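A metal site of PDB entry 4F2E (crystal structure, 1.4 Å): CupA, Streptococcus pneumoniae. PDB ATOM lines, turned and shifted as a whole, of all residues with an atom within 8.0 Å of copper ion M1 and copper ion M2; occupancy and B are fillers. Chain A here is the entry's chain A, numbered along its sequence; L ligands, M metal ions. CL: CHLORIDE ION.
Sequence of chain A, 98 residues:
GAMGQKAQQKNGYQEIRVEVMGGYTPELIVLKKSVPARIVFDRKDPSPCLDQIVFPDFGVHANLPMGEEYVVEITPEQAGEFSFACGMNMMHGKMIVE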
ATOM      1  N   GLY A  23     -11.669   0.993  19.100  1.00  0.00           N
ATOM      2  CA  GLY A  23     -11.679   1.359  20.503  1.00  0.00           C
ATOM      3  C   GLY A  23     -12.887   0.734  21.175  1.00  0.00           C
ATOM      4  O   GLY A  23     -13.369  -0.314  20.739  1.00  0.00           O
ATOM      5  N   TYR A  24     -13.389   1.388  22.212  1.00  0.00           N
ATOM      6  CA  TYR A  24     -14.482   0.844  22.998  1.00  0.00           C
ATOM      7  C   TYR A  24     -15.602   1.856  23.068  1.00  0.00           C
ATOM      8  O   TYR A  24     -15.371   3.030  23.299  1.00  0.00           O
ATOM      9  CB  TYR A  24     -13.981   0.508  24.409  1.00  0.00           C
ATOM     10  CG  TYR A  24     -12.720  -0.320  24.361  1.00  0.00           C
ATOM     11  CD1 TYR A  24     -12.760  -1.642  23.945  1.00  0.00           C
ATOM     12  CD2 TYR A  24     -11.487   0.231  24.679  1.00  0.00           C
ATOM     13  CE1 TYR A  24     -11.616  -2.398  23.862  1.00  0.00           C
ATOM     14  CE2 TYR A  24     -10.331  -0.526  24.603  1.00  0.00           C
ATOM     15  CZ  TYR A  24     -10.405  -1.844  24.190  1.00  0.00           C
ATOM     16  OH  TYR A  24      -9.268  -2.607  24.105  1.00  0.00           O
ATOM     17  N   SER A  47      -8.730  -5.618  13.991  1.00  0.00           N
ATOM     18  CA  SER A  47      -7.388  -5.077  14.126  1.00  0.00           C
ATOM     19  C   SER A  47      -6.627  -5.769  15.241  1.00  0.00           C
ATOM     20  O   SER A  47      -7.136  -5.916  16.361  1.00  0.00           O
ATOM     21  CB  SER A  47      -7.426  -3.580  14.422  1.00  0.00           C
ATOM     22  OG  SER A  47      -6.119  -3.109  14.707  1.00  0.00           O
ATOM     23  N   PRO A  48      -5.386  -6.197  14.957  1.00  0.00           N
ATOM     24  CA  PRO A  48      -4.543  -6.793  16.013  1.00  0.00           C
ATOM     25  C   PRO A  48      -4.363  -5.856  17.208  1.00  0.00           C
ATOM     26  O   PRO A  48      -4.073  -6.330  18.300  1.00  0.00           O
ATOM     27  CB  PRO A  48      -3.211  -7.029  15.289  1.00  0.00           C
ATOM     28  CG  PRO A  48      -3.602  -7.200  13.851  1.00  0.00           C
ATOM     29  CD  PRO A  48      -4.741  -6.253  13.634  1.00  0.00           C
ATOM     30  N   CYS A  49      -4.522  -4.557  16.993  1.00  0.00           N
ATOM     31  CA  CYS A  49      -4.438  -3.612  18.098  1.00  0.00           C
ATOM     32  C   CYS A  49      -5.433  -3.948  19.204  1.00  0.00           C
ATOM     33  O   CYS A  49      -5.210  -3.642  20.376  1.00  0.00           O
ATOM     34  CB  CYS A  49      -4.687  -2.184  17.580  1.00  0.00           C
ATOM     35  SG  CYS A  49      -4.341  -0.847  18.771  1.00  0.00           S
ATOM     36  N   LEU A  50      -6.532  -4.602  18.834  1.00  0.00           N
ATOM     37  CA  LEU A  50      -7.630  -4.871  19.774  1.00  0.00           C
ATOM     38  C   LEU A  50      -7.727  -6.344  20.203  1.00  0.00           C
ATOM     39  O   LEU A  50      -8.781  -6.784  20.671  1.00  0.00           O
ATOM     40  CB  LEU A  50      -8.949  -4.379  19.181  1.00  0.00           C
ATOM     41  CG  LEU A  50      -9.005  -2.865  18.972  1.00  0.00           C
ATOM     42  CD1 LEU A  50     -10.117  -2.477  18.004  1.00  0.00           C
ATOM     43  CD2 LEU A  50      -9.177  -2.141  20.303  1.00  0.00           C
ATOM     44  N   ASP A  51      -6.633  -7.076  20.064  1.00  0.00           N
ATOM     45  CA  ASP A  51      -6.615  -8.510  20.373  1.00  0.00           C
ATOM     46  C   ASP A  51      -6.823  -8.825  21.852  1.00  0.00           C
ATOM     47  O   ASP A  51      -7.319  -9.902  22.199  1.00  0.00           O
ATOM     48  CB  ASP A  51      -5.303  -9.154  19.900  1.00  0.00           C
ATOM     49  CG  ASP A  51      -5.317  -9.458  18.423  1.00  0.00           C
ATOM     50  OD1 ASP A  51      -6.398  -9.381  17.793  1.00  0.00           O
ATOM     51  OD2 ASP A  51      -4.241  -9.785  17.883  1.00  0.00           O
ATOM     52  N   GLN A  52      -6.420  -7.912  22.732  1.00  0.00           N
ATOM     53  CA  GLN A  52      -6.518  -8.146  24.160  1.00  0.00           C
ATOM     54  C   GLN A  52      -7.213  -7.014  24.893  1.00  0.00           C
ATOM     55  O   GLN A  52      -7.223  -5.875  24.438  1.00  0.00           O
ATOM     56  CB  GLN A  52      -5.131  -8.376  24.763  1.00  0.00           C
ATOM     57  CG  GLN A  52      -4.450  -9.652  24.303  1.00  0.00           C
ATOM     58  CD  GLN A  52      -3.193  -9.387  23.511  1.00  0.00           C
ATOM     59  OE1 GLN A  52      -2.395  -8.515  23.872  1.00  0.00           O
ATOM     60  NE2 GLN A  52      -3.000 -10.139  22.432  1.00  0.00           N
ATOM     61  N   ALA A  85      -7.903  -0.851  28.880  1.00  0.00           N
ATOM     62  CA  ALA A  85      -7.228  -0.581  27.623  1.00  0.00           C
ATOM     63  C   ALA A  85      -6.975  -1.858  26.868  1.00  0.00           C
ATOM     64  O   ALA A  85      -7.163  -2.950  27.389  1.00  0.00           O
ATOM     65  CB  ALA A  85      -5.914   0.153  27.883  1.00  0.00           C
ATOM     66  N   CYS A  86      -6.561  -1.719  25.615  1.00  0.00           N
ATOM     67  CA  CYS A  86      -6.155  -2.880  24.834  1.00  0.00           C
ATOM     68  C   CYS A  86      -4.801  -3.354  25.349  1.00  0.00           C
ATOM     69  O   CYS A  86      -4.188  -2.713  26.201  1.00  0.00           O
ATOM     70  CB  CYS A  86      -6.071  -2.530  23.359  1.00  0.00           C
ATOM     71  SG  CYS A  86      -4.683  -1.432  22.964  1.00  0.00           S
ATOM     72  N   GLY A  87      -4.343  -4.488  24.824  1.00  0.00           N
ATOM     73  CA  GLY A  87      -3.080  -5.062  25.255  1.00  0.00           C
ATOM     74  C   GLY A  87      -1.856  -4.210  24.922  1.00  0.00           C
ATOM     75  O   GLY A  87      -0.776  -4.483  25.435  1.00  0.00           O
ATOM     76  N   MET A  88      -2.032  -3.204  24.079  1.00  0.00           N
ATOM     77  CA  MET A  88      -0.938  -2.307  23.687  1.00  0.00           C
ATOM     78  C   MET A  88      -0.976  -0.981  24.433  1.00  0.00           C
ATOM     79  O   MET A  88      -0.091  -0.140  24.243  1.00  0.00           O
ATOM     80  CB  MET A  88      -0.986  -2.019  22.189  1.00  0.00           C
ATOM     81  CG  MET A  88      -0.973  -3.245  21.299  1.00  0.00           C
ATOM     82  SD  MET A  88      -0.798  -2.762  19.574  1.00  0.00           S
ATOM     83  CE  MET A  88       0.893  -2.157  19.548  1.00  0.00           C
ATOM     84  N   ASN A  89      -1.999  -0.777  25.242  1.00  0.00           N
ATOM     85  CA  ASN A  89      -2.207   0.505  25.929  1.00  0.00           C
ATOM     86  C   ASN A  89      -2.342   1.642  24.913  1.00  0.00           C
ATOM     87  O   ASN A  89      -1.878   2.756  25.148  1.00  0.00           O
ATOM     88  CB  ASN A  89      -1.054   0.786  26.898  1.00  0.00           C
ATOM     89  CG  ASN A  89      -1.419   1.800  27.970  1.00  0.00           C
ATOM     90  OD1 ASN A  89      -2.592   1.989  28.291  1.00  0.00           O
ATOM     91  ND2 ASN A  89      -0.405   2.463  28.537  1.00  0.00           N
ATOM     92  N   MET A  90      -3.003   1.353  23.786  1.00  0.00           N
ATOM     93  CA  MET A  90      -3.236   2.350  22.739  1.00  0.00           C
ATOM     94  C   MET A  90      -4.685   2.812  22.701  1.00  0.00           C
ATOM     95  O   MET A  90      -4.959   3.984  22.430  1.00  0.00           O
ATOM     96  CB  MET A  90      -2.855   1.792  21.367  1.00  0.00           C
ATOM     97  CG  MET A  90      -1.369   1.671  21.122  1.00  0.00           C
ATOM     98  SD  MET A  90      -0.953   0.983  19.497  1.00  0.00           S
ATOM     99  CE  MET A  90      -1.681   2.212  18.411  1.00  0.00           C
ATOM    100  N   MET A  91      -5.604   1.885  22.952  1.00  0.00           N
ATOM    101  CA  MET A  91      -7.035   2.188  22.996  1.00  0.00           C
ATOM    102  C   MET A  91      -7.491   2.117  24.443  1.00  0.00           C
ATOM    103  O   MET A  91      -7.118   1.198  25.164  1.00  0.00           O
ATOM    104  CB  MET A  91      -7.809   1.164  22.171  1.00  0.00           C
ATOM    105  CG  MET A  91      -7.304   0.989  20.751  1.00  0.00           C
ATOM    106  SD  MET A  91      -8.068   2.155  19.614  1.00  0.00           S
ATOM    107  CE  MET A  91      -7.188   3.653  19.975  1.00  0.00           C
ATOM    108  N   HIS A  92      -8.327   3.069  24.860  1.00  0.00           N
ATOM    109  CA  HIS A  92      -8.607   3.264  26.283  1.00  0.00           C
ATOM    110  C   HIS A  92     -10.073   3.399  26.652  1.00  0.00           C
ATOM    111  O   HIS A  92     -10.916   3.796  25.855  1.00  0.00           O
ATOM    112  CB  HIS A  92      -7.861   4.506  26.783  1.00  0.00           C
ATOM    113  CG  HIS A  92      -6.415   4.515  26.437  1.00  0.00           C
ATOM    114  ND1 HIS A  92      -5.459   3.883  27.202  1.00  0.00           N
ATOM    115  CD2 HIS A  92      -5.746   5.081  25.410  1.00  0.00           C
ATOM    116  CE1 HIS A  92      -4.269   4.064  26.662  1.00  0.00           C
ATOM    117  NE2 HIS A  92      -4.411   4.782  25.568  1.00  0.00           N
HETATM  118 CL    CL L   1      -1.486  -1.092  16.732  1.00  0.00          CL
HETATM  119 CU    CU M   1      -2.108  -0.957  18.973  1.00  0.00          CU
HETATM  120 CU    CU M   2      -4.608  -1.548  20.790  1.00  0.00          CU
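Copper ion M2 is bound by the side-chain sulfur (SG) of Cys 49 (2.2 Å), the side-chain sulfur (SG) of Cys 86 (2.2 Å) and the backbone carbonyl oxygen (O) of Cys 49 (2.2 Å).
Copper ion M2 has three donor atoms within binding distance.
N of Cys 49 sits close to OG of Ser 47, 3.1 Å away.
SG of Cys 86 sits close to N of Met 88, 3.4 Å away.
SG of Cys 86 lies close to N of Met 90, 3.4 Å away.
The backbone carbonyl oxygen (O) of Met 91 is in hydrogen-bond range of the backbone NH (N) of Cys 86 (3.0 Å).
The side-chain sulfur (SG) of Cys 86 lies close to the backbone NH (N) of Asn 89 (3.6 Å).
The side-chain hydroxyl of Tyr 24 lies close to the backbone NH of Cys 86 (3.2 Å).
O of Met 90 sits close to NE2 of His 92 (3.3 Å).
Merely in contact with copper ion M2: Met 91 (3.7 Å).
Within 4 Å of copper ion M2: Cys 49, Cys 86, Met 88, Met 90 and Met 91.
The nearest printed residue that does not touch copper ion M2 is Leu 50 (4.1 Å).
Copper ion M1 is bound by the side-chain sulfur (SG) of Cys 49.
SD of Met 88 is bound to copper ion M1 (2.3 Å).
Copper ion M1 is bound by SD of Met 90 (2.3 Å).
CL of the ligand binds copper ion M1 (2.3 Å).
Of the 16 residues printed, 3 come within 4 Å of copper ion M1.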
